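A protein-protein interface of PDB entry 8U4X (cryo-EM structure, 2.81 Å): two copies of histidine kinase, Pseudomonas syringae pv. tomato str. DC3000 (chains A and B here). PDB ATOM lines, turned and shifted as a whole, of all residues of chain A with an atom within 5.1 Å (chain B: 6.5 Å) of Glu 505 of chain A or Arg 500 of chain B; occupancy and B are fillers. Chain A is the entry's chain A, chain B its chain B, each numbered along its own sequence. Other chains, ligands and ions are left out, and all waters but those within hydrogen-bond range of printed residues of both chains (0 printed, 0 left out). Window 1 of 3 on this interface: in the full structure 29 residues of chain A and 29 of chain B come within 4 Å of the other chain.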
ATOM      1  N   HIS A 336     -18.528  -4.388   3.213  1.00  0.00           N
ATOM      2  CA  HIS A 336     -19.384  -3.730   4.196  1.00  0.00           C
ATOM      3  C   HIS A 336     -19.278  -2.213   4.087  1.00  0.00           C
ATOM      4  O   HIS A 336     -20.286  -1.501   4.167  1.00  0.00           O
ATOM      5  CB  HIS A 336     -19.014  -4.198   5.604  1.00  0.00           C
ATOM      6  CG  HIS A 336     -19.950  -3.718   6.670  1.00  0.00           C
ATOM      7  ND1 HIS A 336     -19.649  -3.794   8.012  1.00  0.00           N
ATOM      8  CD2 HIS A 336     -21.183  -3.163   6.591  1.00  0.00           C
ATOM      9  CE1 HIS A 336     -20.654  -3.302   8.716  1.00  0.00           C
ATOM     10  NE2 HIS A 336     -21.597  -2.912   7.878  1.00  0.00           N
ATOM     11  N   ARG A 500     -24.359 -11.974   4.508  1.00  0.00           N
ATOM     12  CA  ARG A 500     -25.776 -11.949   4.851  1.00  0.00           C
ATOM     13  C   ARG A 500     -26.024 -11.135   6.116  1.00  0.00           C
ATOM     14  O   ARG A 500     -26.986 -10.364   6.189  1.00  0.00           O
ATOM     15  CB  ARG A 500     -26.304 -13.372   5.022  1.00  0.00           C
ATOM     16  CG  ARG A 500     -27.819 -13.457   5.082  1.00  0.00           C
ATOM     17  CD  ARG A 500     -28.275 -14.628   5.931  1.00  0.00           C
ATOM     18  NE  ARG A 500     -29.715 -14.830   5.843  1.00  0.00           N
ATOM     19  CZ  ARG A 500     -30.562 -14.621   6.841  1.00  0.00           C
ATOM     20  NH1 ARG A 500     -30.145 -14.201   8.025  1.00  0.00           N
ATOM     21  NH2 ARG A 500     -31.859 -14.840   6.648  1.00  0.00           N
ATOM     22  N   ARG A 501     -25.170 -11.304   7.127  1.00  0.00           N
ATOM     23  CA  ARG A 501     -25.327 -10.556   8.374  1.00  0.00           C
ATOM     24  C   ARG A 501     -25.123  -9.059   8.156  1.00  0.00           C
ATOM     25  O   ARG A 501     -25.879  -8.232   8.684  1.00  0.00           O
ATOM     26  CB  ARG A 501     -24.352 -11.093   9.423  1.00  0.00           C
ATOM     27  CG  ARG A 501     -23.800 -10.046  10.378  1.00  0.00           C
ATOM     28  CD  ARG A 501     -22.585 -10.575  11.123  1.00  0.00           C
ATOM     29  NE  ARG A 501     -21.788  -9.505  11.710  1.00  0.00           N
ATOM     30  CZ  ARG A 501     -20.665  -9.694  12.389  1.00  0.00           C
ATOM     31  NH1 ARG A 501     -20.171 -10.906  12.584  1.00  0.00           N
ATOM     32  NH2 ARG A 501     -20.020  -8.641  12.883  1.00  0.00           N
ATOM     33  N   SER A 502     -24.099  -8.694   7.380  1.00  0.00           N
ATOM     34  CA  SER A 502     -23.865  -7.285   7.077  1.00  0.00           C
ATOM     35  C   SER A 502     -25.024  -6.693   6.288  1.00  0.00           C
ATOM     36  O   SER A 502     -25.443  -5.558   6.544  1.00  0.00           O
ATOM     37  CB  SER A 502     -22.552  -7.124   6.312  1.00  0.00           C
ATOM     38  OG  SER A 502     -21.485  -7.765   6.988  1.00  0.00           O
ATOM     39  N   ALA A 503     -25.552  -7.450   5.321  1.00  0.00           N
ATOM     40  CA  ALA A 503     -26.712  -6.992   4.568  1.00  0.00           C
ATOM     41  C   ALA A 503     -27.922  -6.830   5.476  1.00  0.00           C
ATOM     42  O   ALA A 503     -28.687  -5.874   5.330  1.00  0.00           O
ATOM     43  CB  ALA A 503     -27.018  -7.965   3.429  1.00  0.00           C
ATOM     44  N   LEU A 504     -28.109  -7.753   6.421  1.00  0.00           N
ATOM     45  CA  LEU A 504     -29.198  -7.638   7.386  1.00  0.00           C
ATOM     46  C   LEU A 504     -29.087  -6.344   8.182  1.00  0.00           C
ATOM     47  O   LEU A 504     -30.053  -5.577   8.287  1.00  0.00           O
ATOM     48  CB  LEU A 504     -29.183  -8.847   8.322  1.00  0.00           C
ATOM     49  CG  LEU A 504     -30.341  -9.842   8.268  1.00  0.00           C
ATOM     50  CD1 LEU A 504     -30.261 -10.803   9.441  1.00  0.00           C
ATOM     51  CD2 LEU A 504     -31.657  -9.098   8.289  1.00  0.00           C
ATOM     52  N   GLU A 505     -27.904  -6.084   8.742  1.00  0.00           N
ATOM     53  CA  GLU A 505     -27.711  -4.890   9.560  1.00  0.00           C
ATOM     54  C   GLU A 505     -27.928  -3.622   8.740  1.00  0.00           C
ATOM     55  O   GLU A 505     -28.684  -2.723   9.141  1.00  0.00           O
ATOM     56  CB  GLU A 505     -26.310  -4.903  10.171  1.00  0.00           C
ATOM     57  CG  GLU A 505     -26.212  -5.640  11.495  1.00  0.00           C
ATOM     58  CD  GLU A 505     -24.827  -6.200  11.750  1.00  0.00           C
ATOM     59  OE1 GLU A 505     -24.634  -6.858  12.794  1.00  0.00           O
ATOM     60  OE2 GLU A 505     -23.930  -5.980  10.910  1.00  0.00           O
ATOM     61  N   ASN A 506     -27.280  -3.539   7.575  1.00  0.00           N
ATOM     62  CA  ASN A 506     -27.404  -2.355   6.736  1.00  0.00           C
ATOM     63  C   ASN A 506     -28.832  -2.151   6.251  1.00  0.00           C
ATOM     64  O   ASN A 506     -29.324  -1.019   6.249  1.00  0.00           O
ATOM     65  CB  ASN A 506     -26.445  -2.451   5.549  1.00  0.00           C
ATOM     66  CG  ASN A 506     -24.990  -2.370   5.970  1.00  0.00           C
ATOM     67  OD1 ASN A 506     -24.621  -2.824   7.052  1.00  0.00           O
ATOM     68  ND2 ASN A 506     -24.157  -1.794   5.112  1.00  0.00           N
ATOM     69  N   ASP A 507     -29.515  -3.226   5.850  1.00  0.00           N
ATOM     70  CA  ASP A 507     -30.890  -3.107   5.384  1.00  0.00           C
ATOM     71  C   ASP A 507     -31.812  -2.644   6.501  1.00  0.00           C
ATOM     72  O   ASP A 507     -32.690  -1.806   6.271  1.00  0.00           O
ATOM     73  CB  ASP A 507     -31.365  -4.441   4.809  1.00  0.00           C
ATOM     74  CG  ASP A 507     -32.283  -4.266   3.616  1.00  0.00           C
ATOM     75  OD1 ASP A 507     -32.397  -3.129   3.113  1.00  0.00           O
ATOM     76  OD2 ASP A 507     -32.893  -5.266   3.181  1.00  0.00           O
ATOM     77  N   LEU A 508     -31.639  -3.176   7.717  1.00  0.00           N
ATOM     78  CA  LEU A 508     -32.437  -2.681   8.833  1.00  0.00           C
ATOM     79  C   LEU A 508     -32.198  -1.194   9.045  1.00  0.00           C
ATOM     80  O   LEU A 508     -33.147  -0.428   9.261  1.00  0.00           O
ATOM     81  CB  LEU A 508     -32.120  -3.452  10.113  1.00  0.00           C
ATOM     82  CG  LEU A 508     -33.053  -3.086  11.274  1.00  0.00           C
ATOM     83  CD1 LEU A 508     -34.414  -3.754  11.112  1.00  0.00           C
ATOM     84  CD2 LEU A 508     -32.439  -3.401  12.631  1.00  0.00           C
ATOM     85  N   ALA A 509     -30.935  -0.767   8.968  1.00  0.00           N
ATOM     86  CA  ALA A 509     -30.636   0.654   9.111  1.00  0.00           C
ATOM     87  C   ALA A 509     -31.339   1.481   8.039  1.00  0.00           C
ATOM     88  O   ALA A 509     -31.915   2.535   8.337  1.00  0.00           O
ATOM     89  CB  ALA A 509     -29.126   0.880   9.060  1.00  0.00           C
ATOM     90  N   GLU B 398     -20.387  -2.389  20.497  1.00  0.00           N
ATOM     91  CA  GLU B 398     -20.523  -3.835  20.404  1.00  0.00           C
ATOM     92  C   GLU B 398     -21.999  -4.219  20.335  1.00  0.00           C
ATOM     93  O   GLU B 398     -22.819  -3.654  21.067  1.00  0.00           O
ATOM     94  CB  GLU B 398     -19.859  -4.519  21.597  1.00  0.00           C
ATOM     95  CG  GLU B 398     -18.342  -4.429  21.604  1.00  0.00           C
ATOM     96  CD  GLU B 398     -17.731  -4.976  22.878  1.00  0.00           C
ATOM     97  OE1 GLU B 398     -18.496  -5.418  23.763  1.00  0.00           O
ATOM     98  OE2 GLU B 398     -16.489  -4.966  22.997  1.00  0.00           O
ATOM     99  N   PRO B 399     -22.372  -5.159  19.462  1.00  0.00           N
ATOM    100  CA  PRO B 399     -23.781  -5.587  19.407  1.00  0.00           C
ATOM    101  C   PRO B 399     -24.281  -6.183  20.711  1.00  0.00           C
ATOM    102  O   PRO B 399     -25.453  -5.995  21.058  1.00  0.00           O
ATOM    103  CB  PRO B 399     -23.786  -6.620  18.271  1.00  0.00           C
ATOM    104  CG  PRO B 399     -22.373  -7.105  18.192  1.00  0.00           C
ATOM    105  CD  PRO B 399     -21.523  -5.917  18.528  1.00  0.00           C
ATOM    106  N   VAL B 400     -23.429  -6.896  21.441  1.00  0.00           N
ATOM    107  CA  VAL B 400     -23.777  -7.470  22.734  1.00  0.00           C
ATOM    108  C   VAL B 400     -22.653  -7.158  23.712  1.00  0.00           C
ATOM    109  O   VAL B 400     -21.502  -6.962  23.307  1.00  0.00           O
ATOM    110  CB  VAL B 400     -24.023  -8.993  22.637  1.00  0.00           C
ATOM    111  CG1 VAL B 400     -22.708  -9.760  22.634  1.00  0.00           C
ATOM    112  CG2 VAL B 400     -24.923  -9.464  23.770  1.00  0.00           C
ATOM    113  N   MET B 426     -28.023  -6.176  24.997  1.00  0.00           N
ATOM    114  CA  MET B 426     -28.014  -6.416  23.560  1.00  0.00           C
ATOM    115  C   MET B 426     -28.996  -5.463  22.892  1.00  0.00           C
ATOM    116  O   MET B 426     -30.121  -5.284  23.367  1.00  0.00           O
ATOM    117  CB  MET B 426     -28.322  -7.899  23.253  1.00  0.00           C
ATOM    118  CG  MET B 426     -29.785  -8.308  23.052  1.00  0.00           C
ATOM    119  SD  MET B 426     -30.547  -7.855  21.478  1.00  0.00           S
ATOM    120  CE  MET B 426     -32.254  -8.283  21.804  1.00  0.00           C
ATOM    121  N   SER B 427     -28.562  -4.844  21.796  1.00  0.00           N
ATOM    122  CA  SER B 427     -29.346  -3.821  21.119  1.00  0.00           C
ATOM    123  C   SER B 427     -29.356  -4.071  19.619  1.00  0.00           C
ATOM    124  O   SER B 427     -28.390  -4.594  19.056  1.00  0.00           O
ATOM    125  CB  SER B 427     -28.798  -2.417  21.408  1.00  0.00           C
ATOM    126  OG  SER B 427     -27.891  -2.005  20.400  1.00  0.00           O
ATOM    127  N   LEU B 428     -30.461  -3.691  18.978  1.00  0.00           N
ATOM    128  CA  LEU B 428     -30.603  -3.803  17.535  1.00  0.00           C
ATOM    129  C   LEU B 428     -29.811  -2.700  16.833  1.00  0.00           C
ATOM    130  O   LEU B 428     -29.662  -1.600  17.373  1.00  0.00           O
ATOM    131  CB  LEU B 428     -32.071  -3.716  17.132  1.00  0.00           C
ATOM    132  CG  LEU B 428     -32.867  -5.020  17.203  1.00  0.00           C
ATOM    133  CD1 LEU B 428     -34.343  -4.767  16.941  1.00  0.00           C
ATOM    134  CD2 LEU B 428     -32.311  -6.043  16.223  1.00  0.00           C
ATOM    135  N   PRO B 429     -29.295  -2.968  15.632  1.00  0.00           N
ATOM    136  CA  PRO B 429     -28.498  -1.955  14.920  1.00  0.00           C
ATOM    137  C   PRO B 429     -29.357  -0.983  14.118  1.00  0.00           C
ATOM    138  O   PRO B 429     -29.398  -1.019  12.883  1.00  0.00           O
ATOM    139  CB  PRO B 429     -27.605  -2.812  14.020  1.00  0.00           C
ATOM    140  CG  PRO B 429     -28.453  -4.001  13.704  1.00  0.00           C
ATOM    141  CD  PRO B 429     -29.354  -4.241  14.892  1.00  0.00           C
ATOM    142  N   LYS B 430     -30.051  -0.099  14.822  1.00  0.00           N
ATOM    143  CA  LYS B 430     -30.896   0.907  14.201  1.00  0.00           C
ATOM    144  C   LYS B 430     -30.720   2.233  14.923  1.00  0.00           C
ATOM    145  O   LYS B 430     -30.356   2.259  16.103  1.00  0.00           O
ATOM    146  CB  LYS B 430     -32.372   0.485  14.225  1.00  0.00           C
ATOM    147  CG  LYS B 430     -32.825  -0.134  15.536  1.00  0.00           C
ATOM    148  CD  LYS B 430     -34.182  -0.805  15.385  1.00  0.00           C
ATOM    149  CE  LYS B 430     -35.317   0.166  15.662  1.00  0.00           C
ATOM    150  NZ  LYS B 430     -36.620  -0.339  15.144  1.00  0.00           N
ATOM    151  N   ALA B 495     -27.279 -17.035  23.992  1.00  0.00           N
ATOM    152  CA  ALA B 495     -28.708 -16.750  23.971  1.00  0.00           C
ATOM    153  C   ALA B 495     -28.968 -15.286  23.659  1.00  0.00           C
ATOM    154  O   ALA B 495     -29.898 -14.961  22.915  1.00  0.00           O
ATOM    155  CB  ALA B 495     -29.342 -17.134  25.307  1.00  0.00           C
ATOM    156  N   ALA B 496     -28.154 -14.389  24.219  1.00  0.00           N
ATOM    157  CA  ALA B 496     -28.299 -12.970  23.904  1.00  0.00           C
ATOM    158  C   ALA B 496     -28.086 -12.715  22.415  1.00  0.00           C
ATOM    159  O   ALA B 496     -28.862 -11.992  21.777  1.00  0.00           O
ATOM    160  CB  ALA B 496     -27.322 -12.145  24.743  1.00  0.00           C
ATOM    161  N   ASN B 497     -27.045 -13.322  21.837  1.00  0.00           N
ATOM    162  CA  ASN B 497     -26.758 -13.123  20.419  1.00  0.00           C
ATOM    163  C   ASN B 497     -27.840 -13.735  19.536  1.00  0.00           C
ATOM    164  O   ASN B 497     -28.210 -13.157  18.508  1.00  0.00           O
ATOM    165  CB  ASN B 497     -25.389 -13.709  20.077  1.00  0.00           C
ATOM    166  CG  ASN B 497     -24.247 -12.842  20.567  1.00  0.00           C
ATOM    167  OD1 ASN B 497     -23.872 -11.865  19.920  1.00  0.00           O
ATOM    168  ND2 ASN B 497     -23.689 -13.196  21.718  1.00  0.00           N
ATOM    169  N   ASP B 498     -28.354 -14.909  19.912  1.00  0.00           N
ATOM    170  CA  ASP B 498     -29.416 -15.537  19.134  1.00  0.00           C
ATOM    171  C   ASP B 498     -30.704 -14.729  19.206  1.00  0.00           C
ATOM    172  O   ASP B 498     -31.422 -14.603  18.207  1.00  0.00           O
ATOM    173  CB  ASP B 498     -29.647 -16.967  19.620  1.00  0.00           C
ATOM    174  CG  ASP B 498     -29.880 -17.940  18.481  1.00  0.00           C
ATOM    175  OD1 ASP B 498     -30.329 -17.499  17.403  1.00  0.00           O
ATOM    176  OD2 ASP B 498     -29.613 -19.146  18.666  1.00  0.00           O
ATOM    177  N   LEU B 499     -31.012 -14.176  20.381  1.00  0.00           N
ATOM    178  CA  LEU B 499     -32.157 -13.282  20.503  1.00  0.00           C
ATOM    179  C   LEU B 499     -31.968 -12.040  19.646  1.00  0.00           C
ATOM    180  O   LEU B 499     -32.915 -11.563  19.012  1.00  0.00           O
ATOM    181  CB  LEU B 499     -32.369 -12.901  21.968  1.00  0.00           C
ATOM    182  CG  LEU B 499     -33.778 -12.474  22.380  1.00  0.00           C
ATOM    183  CD1 LEU B 499     -34.738 -13.650  22.307  1.00  0.00           C
ATOM    184  CD2 LEU B 499     -33.753 -11.882  23.777  1.00  0.00           C
ATOM    185  N   ARG B 500     -30.745 -11.504  19.608  1.00  0.00           N
ATOM    186  CA  ARG B 500     -30.464 -10.356  18.751  1.00  0.00           C
ATOM    187  C   ARG B 500     -30.668 -10.701  17.280  1.00  0.00           C
ATOM    188  O   ARG B 500     -31.227  -9.905  16.521  1.00  0.00           O
ATOM    189  CB  ARG B 500     -29.040  -9.857  18.989  1.00  0.00           C
ATOM    190  CG  ARG B 500     -28.761  -8.498  18.372  1.00  0.00           C
ATOM    191  CD  ARG B 500     -27.303  -8.358  17.977  1.00  0.00           C
ATOM    192  NE  ARG B 500     -26.986  -6.998  17.559  1.00  0.00           N
ATOM    193  CZ  ARG B 500     -26.677  -6.650  16.318  1.00  0.00           C
ATOM    194  NH1 ARG B 500     -26.634  -7.541  15.341  1.00  0.00           N
ATOM    195  NH2 ARG B 500     -26.402  -5.377  16.050  1.00  0.00           N
ATOM    196  N   ARG B 501     -30.211 -11.881  16.861  1.00  0.00           N
ATOM    197  CA  ARG B 501     -30.373 -12.298  15.470  1.00  0.00           C
ATOM    198  C   ARG B 501     -31.845 -12.488  15.112  1.00  0.00           C
ATOM    199  O   ARG B 501     -32.297 -12.069  14.037  1.00  0.00           O
ATOM    200  CB  ARG B 501     -29.580 -13.582  15.219  1.00  0.00           C
ATOM    201  CG  ARG B 501     -30.214 -14.541  14.224  1.00  0.00           C
ATOM    202  CD  ARG B 501     -29.578 -15.919  14.315  1.00  0.00           C
ATOM    203  NE  ARG B 501     -30.410 -16.952  13.709  1.00  0.00           N
ATOM    204  CZ  ARG B 501     -30.098 -18.240  13.679  1.00  0.00           C
ATOM    205  NH1 ARG B 501     -28.976 -18.694  14.213  1.00  0.00           N
ATOM    206  NH2 ARG B 501     -30.933 -19.096  13.096  1.00  0.00           N
ATOM    207  N   SER B 502     -32.608 -13.124  16.005  1.00  0.00           N
ATOM    208  CA  SER B 502     -34.036 -13.302  15.765  1.00  0.00           C
ATOM    209  C   SER B 502     -34.754 -11.961  15.708  1.00  0.00           C
ATOM    210  O   SER B 502     -35.636 -11.756  14.863  1.00  0.00           O
ATOM    211  CB  SER B 502     -34.644 -14.192  16.850  1.00  0.00           C
ATOM    212  OG  SER B 502     -33.915 -15.401  16.983  1.00  0.00           O
ATOM    213  N   ALA B 503     -34.391 -11.036  16.602  1.00  0.00           N
ATOM    214  CA  ALA B 503     -34.973  -9.701  16.568  1.00  0.00           C
ATOM    215  C   ALA B 503     -34.614  -8.982  15.276  1.00  0.00           C
ATOM    216  O   ALA B 503     -35.452  -8.287  14.697  1.00  0.00           O
ATOM    217  CB  ALA B 503     -34.508  -8.894  17.780  1.00  0.00           C
ATOM    218  N   LEU B 504     -33.376  -9.142  14.808  1.00  0.00           N
ATOM    219  CA  LEU B 504     -32.967  -8.554  13.536  1.00  0.00           C
ATOM    220  C   LEU B 504     -33.836  -9.063  12.393  1.00  0.00           C
ATOM    221  O   LEU B 504     -34.379  -8.275  11.607  1.00  0.00           O
ATOM    222  CB  LEU B 504     -31.494  -8.875  13.272  1.00  0.00           C
ATOM    223  CG  LEU B 504     -30.476  -7.738  13.266  1.00  0.00           C
ATOM    224  CD1 LEU B 504     -29.142  -8.230  12.733  1.00  0.00           C
ATOM    225  CD2 LEU B 504     -30.988  -6.595  12.418  1.00  0.00           C
ATOM    226  N   GLU B 505     -33.987 -10.385  12.299  1.00  0.00           N
ATOM    227  CA  GLU B 505     -34.769 -10.971  11.212  1.00  0.00           C
ATOM    228  C   GLU B 505     -36.224 -10.517  11.276  1.00  0.00           C
ATOM    229  O   GLU B 505     -36.790 -10.050  10.275  1.00  0.00           O
ATOM    230  CB  GLU B 505     -34.677 -12.497  11.275  1.00  0.00           C
ATOM    231  CG  GLU B 505     -33.489 -13.082  10.533  1.00  0.00           C
ATOM    232  CD  GLU B 505     -33.039 -14.411  11.105  1.00  0.00           C
ATOM    233  OE1 GLU B 505     -32.048 -14.974  10.598  1.00  0.00           O
ATOM    234  OE2 GLU B 505     -33.682 -14.897  12.060  1.00  0.00           O
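The side-chain carboxylate (OE1) of Glu 505 of chain A lies within salt-bridge range of the guanidinium group (NH1) of Arg 500 of chain B, at 3.3 Å.
The side-chain carboxylate (OE1) of Glu 505 of chain B lies within salt-bridge range of the guanidinium group (NH1) of Arg 500 of chain A (3.3 Å).
The backbone carbonyl oxygen (O) of Ser 427 of chain B lies within hydrogen-bond range of the guanidinium group (NE) of Arg 500 of chain B (3.2 Å).
Glu 505 of chain A touches Pro 429 of chain B.
O of Pro 429 of chain B touches CD2 of Leu 508 of chain A (3.9 Å).
CD2 of Leu 508 of chain A touches CD2 of Leu 504 of chain B, at 3.5 Å.
Arg 500 of chain B touches one residue of chain A.
Of the printed residues of chain B, Arg 500 of chain A touches Glu 505.
Of the printed residues of chain A, Glu 505 of chain B touches Arg 500 (3.3 Å).
Printed residues of chain B within 4 Å of Leu 508 of chain A: Pro 429 (3.9 Å) and Leu 504 (3.5 Å).
The nearest residue of chain B that does not touch Glu 505 of chain A is Leu 504 of chain B (4.1 Å).
The nearest printed residue of chain A that does not touch Arg 500 of chain B is Arg 501 of chain A (6.2 Å).
Of the 11 printed residues of chain A, 3 touch a printed residue of chain B.
Hydrophobic or aromatic side chains of chain A that line the printed part of chain B: Leu 508.
Hydrophobic or aromatic side chains of chain B that line the printed part of chain A: Pro 429 and Leu 504.
Among the printed residues, 5 pairs touch across the chains.
Arg 500 of chain A touches Glu 505 of chain B, and with the chains exchanged Glu 505 of chain A touches Arg 500 of chain B.
Positions printed for both chains: 500, 501, 502, 503, 504 and 505.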
